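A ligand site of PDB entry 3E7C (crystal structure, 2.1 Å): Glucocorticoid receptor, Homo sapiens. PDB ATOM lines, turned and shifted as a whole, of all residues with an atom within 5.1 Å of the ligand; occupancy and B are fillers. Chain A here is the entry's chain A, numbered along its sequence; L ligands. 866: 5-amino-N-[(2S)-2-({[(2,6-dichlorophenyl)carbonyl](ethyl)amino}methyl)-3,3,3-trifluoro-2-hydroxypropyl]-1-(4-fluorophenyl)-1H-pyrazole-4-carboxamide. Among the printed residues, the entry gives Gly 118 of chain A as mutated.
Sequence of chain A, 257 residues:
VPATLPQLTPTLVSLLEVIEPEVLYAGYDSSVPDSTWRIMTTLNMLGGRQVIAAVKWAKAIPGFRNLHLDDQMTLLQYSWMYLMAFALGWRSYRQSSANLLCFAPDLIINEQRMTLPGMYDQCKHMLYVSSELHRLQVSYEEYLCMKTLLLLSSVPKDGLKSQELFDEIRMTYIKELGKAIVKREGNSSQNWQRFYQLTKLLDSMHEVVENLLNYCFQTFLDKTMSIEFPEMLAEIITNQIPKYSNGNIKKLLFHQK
The backbone carbonyl oxygen (O) of Gly 118 is in hydrogen-bond range of the side-chain hydroxyl (OH) of Tyr 215 (2.6 Å).
The backbone carbonyl oxygen of Tyr 215 is in hydrogen-bond range of the side-chain hydroxyl of Thr 219 (3.0 Å).
NE2 of Gln 122 is in hydrogen-bond range of O of Leu 212.
OD1 of Asn 44 sits close to O of Met 40, 3.2 Å away.
The backbone carbonyl oxygen (O) of Ala 87 sits close to a fluorine (F1) of the ligand, at 3.4 Å.
The guanidinium group of Arg 91 lies close to a fluorine (F1) of the ligand (2.9 Å).
Residues that only touch the ligand: Tyr 215, Cys 216, Phe 103, Met 81, Leu 233, Met 126, Trp 80, Gly 47, Gly 118, Met 40, Thr 219, Leu 88 and Phe 229.
Hydrophobic or aromatic side chains that line the ligand: Leu 43, Trp 80, Met 81, Met 84, Ala 87, Leu 88, Phe 103, Met 126, Tyr 215, Phe 229 and Leu 233.
20 residues have an atom within 4 Å of the ligand: Met 40, Leu 43, Asn 44, Gly 47, Gln 50, Trp 80, Met 81, Met 84, Ala 87, Leu 88, Arg 91, Phe 103, Gly 118, Gln 122, Met 126, Tyr 215, Cys 216, Thr 219, Phe 229 and Leu 233.
NE2 of Gln 122 sits at hydrogen-bond distance from O3 of the ligand, at 2.7 Å.
The backbone NH (N) of Asn 44 is in hydrogen-bond range of an oxygen (O1) of the ligand, 3.0 Å away.
The side-chain amide oxygen of Asn 44 is in hydrogen-bond range of an oxygen (O1) of the ligand (2.7 Å).
O1 of the ligand lies close to O of Leu 43 (3.0 Å).
NE2 of Gln 50 sits close to N3 of the ligand, 3.3 Å away.
O of Met 84 lies within hydrogen-bond range of N5 of the ligand, at 3.3 Å.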
ATOM      1  N   MET A  40      -5.446  19.583 -14.518  1.00  0.00           N
ATOM      2  CA  MET A  40      -5.459  18.603 -13.432  1.00  0.00           C
ATOM      3  C   MET A  40      -5.069  19.248 -12.112  1.00  0.00           C
ATOM      4  O   MET A  40      -5.658  18.961 -11.077  1.00  0.00           O
ATOM      5  CB  MET A  40      -4.510  17.441 -13.733  1.00  0.00           C
ATOM      6  CG  MET A  40      -4.941  16.582 -14.920  1.00  0.00           C
ATOM      7  SD  MET A  40      -4.001  15.047 -15.001  1.00  0.00           S
ATOM      8  CE  MET A  40      -2.346  15.679 -15.204  1.00  0.00           C
ATOM      9  N   LEU A  43      -7.602  22.000 -10.904  1.00  0.00           N
ATOM     10  CA  LEU A  43      -8.807  21.284 -10.493  1.00  0.00           C
ATOM     11  C   LEU A  43      -8.638  20.553  -9.148  1.00  0.00           C
ATOM     12  O   LEU A  43      -9.575  20.472  -8.359  1.00  0.00           O
ATOM     13  CB  LEU A  43      -9.255  20.298 -11.580  1.00  0.00           C
ATOM     14  CG  LEU A  43      -9.959  20.948 -12.779  1.00  0.00           C
ATOM     15  CD1 LEU A  43     -10.561  19.892 -13.701  1.00  0.00           C
ATOM     16  CD2 LEU A  43     -11.040  21.919 -12.327  1.00  0.00           C
ATOM     17  N   ASN A  44      -7.453  20.012  -8.918  1.00  0.00           N
ATOM     18  CA  ASN A  44      -7.107  19.459  -7.614  1.00  0.00           C
ATOM     19  C   ASN A  44      -7.216  20.526  -6.538  1.00  0.00           C
ATOM     20  O   ASN A  44      -7.719  20.270  -5.448  1.00  0.00           O
ATOM     21  CB  ASN A  44      -5.684  18.896  -7.614  1.00  0.00           C
ATOM     22  CG  ASN A  44      -5.594  17.531  -8.282  1.00  0.00           C
ATOM     23  OD1 ASN A  44      -6.599  16.971  -8.718  1.00  0.00           O
ATOM     24  ND2 ASN A  44      -4.368  16.997  -8.361  1.00  0.00           N
ATOM     25  N   LEU A  46      -8.964  23.522  -6.582  1.00  0.00           N
ATOM     26  CA  LEU A  46     -10.356  23.868  -6.413  1.00  0.00           C
ATOM     27  C   LEU A  46     -11.113  22.725  -5.738  1.00  0.00           C
ATOM     28  O   LEU A  46     -11.966  22.946  -4.859  1.00  0.00           O
ATOM     29  CB  LEU A  46     -11.004  24.203  -7.761  1.00  0.00           C
ATOM     30  CG  LEU A  46     -12.483  24.606  -7.756  1.00  0.00           C
ATOM     31  CD1 LEU A  46     -12.715  25.882  -6.954  1.00  0.00           C
ATOM     32  CD2 LEU A  46     -12.918  24.813  -9.163  1.00  0.00           C
ATOM     33  N   GLY A  47     -10.805  21.500  -6.141  1.00  0.00           N
ATOM     34  CA  GLY A  47     -11.493  20.329  -5.616  1.00  0.00           C
ATOM     35  C   GLY A  47     -11.304  20.180  -4.113  1.00  0.00           C
ATOM     36  O   GLY A  47     -12.270  19.957  -3.382  1.00  0.00           O
ATOM     37  N   GLY A  48     -10.069  20.315  -3.659  1.00  0.00           N
ATOM     38  CA  GLY A  48      -9.792  20.260  -2.234  1.00  0.00           C
ATOM     39  C   GLY A  48     -10.668  21.242  -1.484  1.00  0.00           C
ATOM     40  O   GLY A  48     -11.180  20.952  -0.405  1.00  0.00           O
ATOM     41  N   GLN A  50     -13.646  22.425  -2.554  1.00  0.00           N
ATOM     42  CA  GLN A  50     -15.049  22.034  -2.687  1.00  0.00           C
ATOM     43  C   GLN A  50     -15.395  20.989  -1.635  1.00  0.00           C
ATOM     44  O   GLN A  50     -16.498  20.951  -1.120  1.00  0.00           O
ATOM     45  CB  GLN A  50     -15.327  21.468  -4.075  1.00  0.00           C
ATOM     46  CG  GLN A  50     -14.842  22.327  -5.250  1.00  0.00           C
ATOM     47  CD  GLN A  50     -15.921  23.227  -5.852  1.00  0.00           C
ATOM     48  OE1 GLN A  50     -16.760  23.783  -5.135  1.00  0.00           O
ATOM     49  NE2 GLN A  50     -15.890  23.372  -7.175  1.00  0.00           N
ATOM     50  N   TRP A  80     -17.477  11.983  -1.100  1.00  0.00           N
ATOM     51  CA  TRP A  80     -16.992  13.270  -1.625  1.00  0.00           C
ATOM     52  C   TRP A  80     -17.072  13.381  -3.146  1.00  0.00           C
ATOM     53  O   TRP A  80     -17.535  14.390  -3.684  1.00  0.00           O
ATOM     54  CB  TRP A  80     -15.577  13.628  -1.132  1.00  0.00           C
ATOM     55  CG  TRP A  80     -14.509  12.719  -1.659  1.00  0.00           C
ATOM     56  CD1 TRP A  80     -14.160  11.486  -1.177  1.00  0.00           C
ATOM     57  CD2 TRP A  80     -13.649  12.985  -2.764  1.00  0.00           C
ATOM     58  NE1 TRP A  80     -13.139  10.963  -1.932  1.00  0.00           N
ATOM     59  CE2 TRP A  80     -12.792  11.860  -2.903  1.00  0.00           C
ATOM     60  CE3 TRP A  80     -13.491  14.055  -3.638  1.00  0.00           C
ATOM     61  CZ2 TRP A  80     -11.816  11.788  -3.880  1.00  0.00           C
ATOM     62  CZ3 TRP A  80     -12.506  13.980  -4.629  1.00  0.00           C
ATOM     63  CH2 TRP A  80     -11.686  12.854  -4.742  1.00  0.00           C
ATOM     64  N   MET A  81     -16.633  12.335  -3.854  1.00  0.00           N
ATOM     65  CA  MET A  81     -16.601  12.438  -5.302  1.00  0.00           C
ATOM     66  C   MET A  81     -18.002  12.335  -5.912  1.00  0.00           C
ATOM     67  O   MET A  81     -18.241  12.833  -7.028  1.00  0.00           O
ATOM     68  CB  MET A  81     -15.645  11.409  -5.927  1.00  0.00           C
ATOM     69  CG  MET A  81     -15.655  11.406  -7.458  1.00  0.00           C
ATOM     70  SD  MET A  81     -15.205  12.999  -8.193  1.00  0.00           S
ATOM     71  CE  MET A  81     -13.412  12.861  -8.219  1.00  0.00           C
ATOM     72  N   LEU A  83     -20.622  13.699  -4.519  1.00  0.00           N
ATOM     73  CA  LEU A  83     -21.106  15.063  -4.341  1.00  0.00           C
ATOM     74  C   LEU A  83     -20.437  16.019  -5.351  1.00  0.00           C
ATOM     75  O   LEU A  83     -21.076  16.955  -5.858  1.00  0.00           O
ATOM     76  CB  LEU A  83     -20.775  15.536  -2.909  1.00  0.00           C
ATOM     77  CG  LEU A  83     -21.264  14.702  -1.708  1.00  0.00           C
ATOM     78  CD1 LEU A  83     -20.683  15.221  -0.373  1.00  0.00           C
ATOM     79  CD2 LEU A  83     -22.778  14.675  -1.675  1.00  0.00           C
ATOM     80  N   MET A  84     -19.147  15.803  -5.615  1.00  0.00           N
ATOM     81  CA  MET A  84     -18.415  16.680  -6.530  1.00  0.00           C
ATOM     82  C   MET A  84     -19.018  16.489  -7.904  1.00  0.00           C
ATOM     83  O   MET A  84     -19.319  17.438  -8.613  1.00  0.00           O
ATOM     84  CB  MET A  84     -16.938  16.284  -6.598  1.00  0.00           C
ATOM     85  CG  MET A  84     -16.143  16.413  -5.311  1.00  0.00           C
ATOM     86  SD  MET A  84     -15.456  18.079  -5.188  1.00  0.00           S
ATOM     87  CE  MET A  84     -16.836  18.746  -4.257  1.00  0.00           C
ATOM     88  N   ALA A  85     -19.137  15.233  -8.287  1.00  0.00           N
ATOM     89  CA  ALA A  85     -19.576  14.875  -9.618  1.00  0.00           C
ATOM     90  C   ALA A  85     -21.015  15.318  -9.843  1.00  0.00           C
ATOM     91  O   ALA A  85     -21.363  15.772 -10.930  1.00  0.00           O
ATOM     92  CB  ALA A  85     -19.457  13.375  -9.824  1.00  0.00           C
ATOM     93  N   ALA A  87     -22.724  17.712  -8.212  1.00  0.00           N
ATOM     94  CA  ALA A  87     -22.813  19.167  -8.154  1.00  0.00           C
ATOM     95  C   ALA A  87     -22.296  19.825  -9.442  1.00  0.00           C
ATOM     96  O   ALA A  87     -22.851  20.838  -9.898  1.00  0.00           O
ATOM     97  CB  ALA A  87     -22.064  19.722  -6.928  1.00  0.00           C
ATOM     98  N   LEU A  88     -21.254  19.223 -10.019  1.00  0.00           N
ATOM     99  CA  LEU A  88     -20.721  19.666 -11.317  1.00  0.00           C
ATOM    100  C   LEU A  88     -21.772  19.414 -12.405  1.00  0.00           C
ATOM    101  O   LEU A  88     -22.098  20.302 -13.177  1.00  0.00           O
ATOM    102  CB  LEU A  88     -19.409  18.939 -11.650  1.00  0.00           C
ATOM    103  CG  LEU A  88     -18.819  19.112 -13.059  1.00  0.00           C
ATOM    104  CD1 LEU A  88     -18.437  20.552 -13.338  1.00  0.00           C
ATOM    105  CD2 LEU A  88     -17.599  18.210 -13.277  1.00  0.00           C
ATOM    106  N   ARG A  91     -24.412  22.107 -12.106  1.00  0.00           N
ATOM    107  CA  ARG A  91     -23.872  23.359 -12.626  1.00  0.00           C
ATOM    108  C   ARG A  91     -23.776  23.364 -14.144  1.00  0.00           C
ATOM    109  O   ARG A  91     -24.110  24.348 -14.792  1.00  0.00           O
ATOM    110  CB  ARG A  91     -22.477  23.584 -12.053  1.00  0.00           C
ATOM    111  CG  ARG A  91     -22.476  24.134 -10.671  1.00  0.00           C
ATOM    112  CD  ARG A  91     -22.324  25.646 -10.684  1.00  0.00           C
ATOM    113  NE  ARG A  91     -22.017  26.088  -9.333  1.00  0.00           N
ATOM    114  CZ  ARG A  91     -20.857  25.856  -8.739  1.00  0.00           C
ATOM    115  NH1 ARG A  91     -19.879  25.238  -9.389  1.00  0.00           N
ATOM    116  NH2 ARG A  91     -20.663  26.268  -7.486  1.00  0.00           N
ATOM    117  N   CYS A 102     -18.724  22.825 -16.409  1.00  0.00           N
ATOM    118  CA  CYS A 102     -18.462  24.126 -15.818  1.00  0.00           C
ATOM    119  C   CYS A 102     -17.865  23.989 -14.415  1.00  0.00           C
ATOM    120  O   CYS A 102     -18.522  24.294 -13.423  1.00  0.00           O
ATOM    121  CB  CYS A 102     -19.744  24.969 -15.799  1.00  0.00           C
ATOM    122  SG  CYS A 102     -20.589  24.992 -17.406  1.00  0.00           S
ATOM    123  N   PHE A 103     -16.623  23.521 -14.352  1.00  0.00           N
ATOM    124  CA  PHE A 103     -15.948  23.310 -13.077  1.00  0.00           C
ATOM    125  C   PHE A 103     -15.962  24.556 -12.205  1.00  0.00           C
ATOM    126  O   PHE A 103     -16.049  24.473 -10.982  1.00  0.00           O
ATOM    127  CB  PHE A 103     -14.524  22.809 -13.288  1.00  0.00           C
ATOM    128  CG  PHE A 103     -14.426  21.330 -13.559  1.00  0.00           C
ATOM    129  CD1 PHE A 103     -14.422  20.848 -14.859  1.00  0.00           C
ATOM    130  CD2 PHE A 103     -14.329  20.431 -12.510  1.00  0.00           C
ATOM    131  CE1 PHE A 103     -14.311  19.493 -15.109  1.00  0.00           C
ATOM    132  CE2 PHE A 103     -14.219  19.061 -12.751  1.00  0.00           C
ATOM    133  CZ  PHE A 103     -14.218  18.595 -14.069  1.00  0.00           C
ATOM    134  N   GLY A 118      -5.648  13.055 -22.622  1.00  0.00           N
ATOM    135  CA  GLY A 118      -6.078  12.365 -21.407  1.00  0.00           C
ATOM    136  C   GLY A 118      -7.191  13.048 -20.638  1.00  0.00           C
ATOM    137  O   GLY A 118      -7.361  12.806 -19.455  1.00  0.00           O
ATOM    138  N   MET A 119      -7.959  13.898 -21.309  1.00  0.00           N
ATOM    139  CA  MET A 119      -8.984  14.691 -20.629  1.00  0.00           C
ATOM    140  C   MET A 119     -10.384  14.126 -20.783  1.00  0.00           C
ATOM    141  O   MET A 119     -11.185  14.172 -19.849  1.00  0.00           O
ATOM    142  CB  MET A 119      -8.955  16.129 -21.144  1.00  0.00           C
ATOM    143  CG  MET A 119      -9.728  17.107 -20.274  1.00  0.00           C
ATOM    144  SD  MET A 119      -8.781  17.577 -18.813  1.00  0.00           S
ATOM    145  CE  MET A 119      -7.246  18.096 -19.568  1.00  0.00           C
ATOM    146  N   GLN A 122     -12.060  11.191 -18.539  1.00  0.00           N
ATOM    147  CA  GLN A 122     -12.583  11.487 -17.211  1.00  0.00           C
ATOM    148  C   GLN A 122     -13.854  12.285 -17.365  1.00  0.00           C
ATOM    149  O   GLN A 122     -14.873  11.981 -16.742  1.00  0.00           O
ATOM    150  CB  GLN A 122     -11.584  12.290 -16.384  1.00  0.00           C
ATOM    151  CG  GLN A 122     -12.050  12.562 -14.963  1.00  0.00           C
ATOM    152  CD  GLN A 122     -11.859  11.356 -14.076  1.00  0.00           C
ATOM    153  OE1 GLN A 122     -12.044  10.226 -14.526  1.00  0.00           O
ATOM    154  NE2 GLN A 122     -11.468  11.579 -12.817  1.00  0.00           N
ATOM    155  N   MET A 126     -18.302  12.740 -16.110  1.00  0.00           N
ATOM    156  CA  MET A 126     -18.980  13.938 -15.655  1.00  0.00           C
ATOM    157  C   MET A 126     -20.091  14.309 -16.611  1.00  0.00           C
ATOM    158  O   MET A 126     -21.171  14.680 -16.188  1.00  0.00           O
ATOM    159  CB  MET A 126     -17.996  15.097 -15.520  1.00  0.00           C
ATOM    160  CG  MET A 126     -16.984  14.913 -14.424  1.00  0.00           C
ATOM    161  SD  MET A 126     -17.752  14.386 -12.876  1.00  0.00           S
ATOM    162  CE  MET A 126     -16.358  14.729 -11.788  1.00  0.00           C
ATOM    163  N   LEU A 212     -14.521   7.670 -12.168  1.00  0.00           N
ATOM    164  CA  LEU A 212     -13.875   8.915 -11.785  1.00  0.00           C
ATOM    165  C   LEU A 212     -12.737   8.639 -10.807  1.00  0.00           C
ATOM    166  O   LEU A 212     -11.652   9.187 -10.938  1.00  0.00           O
ATOM    167  CB  LEU A 212     -14.871   9.876 -11.140  1.00  0.00           C
ATOM    168  CG  LEU A 212     -15.985  10.391 -12.056  1.00  0.00           C
ATOM    169  CD1 LEU A 212     -16.937  11.258 -11.256  1.00  0.00           C
ATOM    170  CD2 LEU A 212     -15.378  11.171 -13.203  1.00  0.00           C
ATOM    171  N   TYR A 215      -9.410   6.859 -12.095  1.00  0.00           N
ATOM    172  CA  TYR A 215      -8.560   7.682 -12.924  1.00  0.00           C
ATOM    173  C   TYR A 215      -8.019   8.861 -12.125  1.00  0.00           C
ATOM    174  O   TYR A 215      -7.041   9.499 -12.528  1.00  0.00           O
ATOM    175  CB  TYR A 215      -9.328   8.136 -14.164  1.00  0.00           C
ATOM    176  CG  TYR A 215      -8.504   8.881 -15.187  1.00  0.00           C
ATOM    177  CD1 TYR A 215      -7.134   8.618 -15.326  1.00  0.00           C
ATOM    178  CD2 TYR A 215      -9.080   9.818 -16.024  1.00  0.00           C
ATOM    179  CE1 TYR A 215      -6.385   9.293 -16.261  1.00  0.00           C
ATOM    180  CE2 TYR A 215      -8.331  10.493 -16.959  1.00  0.00           C
ATOM    181  CZ  TYR A 215      -6.990  10.233 -17.075  1.00  0.00           C
ATOM    182  OH  TYR A 215      -6.241  10.909 -18.010  1.00  0.00           O
ATOM    183  N   CYS A 216      -8.656   9.147 -11.002  1.00  0.00           N
ATOM    184  CA  CYS A 216      -8.141  10.151 -10.071  1.00  0.00           C
ATOM    185  C   CYS A 216      -7.115   9.502  -9.135  1.00  0.00           C
ATOM    186  O   CYS A 216      -6.086  10.103  -8.801  1.00  0.00           O
ATOM    187  CB  CYS A 216      -9.276  10.753  -9.249  1.00  0.00           C
ATOM    188  SG  CYS A 216      -8.707  11.661  -7.797  1.00  0.00           S
ATOM    189  N   THR A 219      -3.867   8.484 -11.018  1.00  0.00           N
ATOM    190  CA  THR A 219      -3.183   9.744 -11.280  1.00  0.00           C
ATOM    191  C   THR A 219      -2.470  10.231 -10.025  1.00  0.00           C
ATOM    192  O   THR A 219      -1.393  10.835 -10.092  1.00  0.00           O
ATOM    193  CB  THR A 219      -4.171  10.818 -11.768  1.00  0.00           C
ATOM    194  OG1 THR A 219      -4.389  10.643 -13.168  1.00  0.00           O
ATOM    195  CG2 THR A 219      -3.630  12.208 -11.531  1.00  0.00           C
ATOM    196  N   PHE A 229      -1.771  17.589  -5.345  1.00  0.00           N
ATOM    197  CA  PHE A 229      -3.073  17.481  -4.691  1.00  0.00           C
ATOM    198  C   PHE A 229      -2.992  18.241  -3.371  1.00  0.00           C
ATOM    199  O   PHE A 229      -2.021  18.115  -2.644  1.00  0.00           O
ATOM    200  CB  PHE A 229      -3.407  16.010  -4.391  1.00  0.00           C
ATOM    201  CG  PHE A 229      -3.807  15.214  -5.595  1.00  0.00           C
ATOM    202  CD1 PHE A 229      -2.838  14.654  -6.419  1.00  0.00           C
ATOM    203  CD2 PHE A 229      -5.144  15.012  -5.895  1.00  0.00           C
ATOM    204  CE1 PHE A 229      -3.201  13.915  -7.533  1.00  0.00           C
ATOM    205  CE2 PHE A 229      -5.515  14.269  -7.006  1.00  0.00           C
ATOM    206  CZ  PHE A 229      -4.542  13.723  -7.831  1.00  0.00           C
ATOM    207  N   LEU A 233      -7.257  16.799   0.411  1.00  0.00           N
ATOM    208  CA  LEU A 233      -7.630  15.818  -0.586  1.00  0.00           C
ATOM    209  C   LEU A 233      -6.697  14.624  -0.612  1.00  0.00           C
ATOM    210  O   LEU A 233      -7.131  13.490  -0.797  1.00  0.00           O
ATOM    211  CB  LEU A 233      -7.662  16.470  -1.964  1.00  0.00           C
ATOM    212  CG  LEU A 233      -8.951  16.308  -2.747  1.00  0.00           C
ATOM    213  CD1 LEU A 233      -8.860  17.039  -4.058  1.00  0.00           C
ATOM    214  CD2 LEU A 233      -9.213  14.844  -2.977  1.00  0.00           C
ATOM    215  N   ILE A 237      -7.763  10.639  -0.224  1.00  0.00           N
ATOM    216  CA  ILE A 237      -7.422   9.745  -1.320  1.00  0.00           C
ATOM    217  C   ILE A 237      -6.581   8.550  -0.829  1.00  0.00           C
ATOM    218  O   ILE A 237      -6.860   7.410  -1.188  1.00  0.00           O
ATOM    219  CB  ILE A 237      -6.697  10.499  -2.442  1.00  0.00           C
ATOM    220  CG1 ILE A 237      -7.656  11.522  -3.057  1.00  0.00           C
ATOM    221  CG2 ILE A 237      -6.197   9.528  -3.504  1.00  0.00           C
ATOM    222  CD1 ILE A 237      -7.122  12.235  -4.280  1.00  0.00           C
HETATM  223  C1  866 L   1      -6.561  14.599 -11.508  1.00  0.00           C
HETATM  224  C2  866 L   1      -7.522  15.737 -11.716  1.00  0.00           C
HETATM  225  N1  866 L   1      -8.826  15.348 -11.258  1.00  0.00           N
HETATM  226  C3  866 L   1      -8.978  15.301  -9.830  1.00  0.00           C
HETATM  227  C4  866 L   1      -9.852  16.389  -9.286  1.00  0.00           C
HETATM  228  O1  866 L   1      -9.155  17.614  -9.330  1.00  0.00           O
HETATM  229  C5  866 L   1     -11.132  16.539 -10.080  1.00  0.00           C
HETATM  230  N2  866 L   1     -11.915  17.617  -9.563  1.00  0.00           N
HETATM  231  C6  866 L   1     -13.274  17.569  -9.727  1.00  0.00           C
HETATM  232  O2  866 L   1     -13.902  16.625 -10.147  1.00  0.00           O
HETATM  233  C7  866 L   1     -13.909  18.773  -9.344  1.00  0.00           C
HETATM  234  C8  866 L   1     -13.364  20.002  -8.900  1.00  0.00           C
HETATM  235  N3  866 L   1     -14.321  20.896  -8.617  1.00  0.00           N
HETATM  236  N4  866 L   1     -15.460  20.238  -8.879  1.00  0.00           N
HETATM  237  C9  866 L   1     -15.255  18.965  -9.311  1.00  0.00           C
HETATM  238  N5  866 L   1     -16.294  18.167  -9.598  1.00  0.00           N
HETATM  239  C10 866 L   1     -16.698  20.844  -8.754  1.00  0.00           C
HETATM  240  C11 866 L   1     -17.096  21.769  -9.676  1.00  0.00           C
HETATM  241  C12 866 L   1     -18.330  22.359  -9.533  1.00  0.00           C
HETATM  242  C13 866 L   1     -19.130  22.011  -8.483  1.00  0.00           C
HETATM  243  F1  866 L   1     -20.329  22.582  -8.335  1.00  0.00           F
HETATM  244  C14 866 L   1     -18.724  21.091  -7.563  1.00  0.00           C
HETATM  245  C15 866 L   1     -17.494  20.495  -7.695  1.00  0.00           C
HETATM  246  C16 866 L   1     -10.162  16.090  -7.845  1.00  0.00           C
HETATM  247  F2  866 L   1     -10.573  17.185  -7.186  1.00  0.00           F
HETATM  248  F3  866 L   1     -11.143  15.176  -7.735  1.00  0.00           F
HETATM  249  F4  866 L   1      -9.080  15.594  -7.229  1.00  0.00           F
HETATM  250  C17 866 L   1      -9.506  14.421 -12.003  1.00  0.00           C
HETATM  251  O3  866 L   1     -10.413  13.713 -11.605  1.00  0.00           O
HETATM  252  C18 866 L   1      -9.080  14.292 -13.391  1.00  0.00           C
HETATM  253  C19 866 L   1      -9.391  15.262 -14.300  1.00  0.00           C
HETATM  254 CL1  866 L   1     -10.269  16.657 -13.848  1.00  0.00          CL
HETATM  255  C20 866 L   1      -9.004  15.126 -15.607  1.00  0.00           C
HETATM  256  C21 866 L   1      -8.307  14.020 -16.005  1.00  0.00           C
HETATM  257  C22 866 L   1      -7.992  13.041 -15.097  1.00  0.00           C
HETATM  258  C23 866 L   1      -8.387  13.173 -13.788  1.00  0.00           C
HETATM  259 CL2  866 L   1      -7.978  11.941 -12.688  1.00  0.00          CL
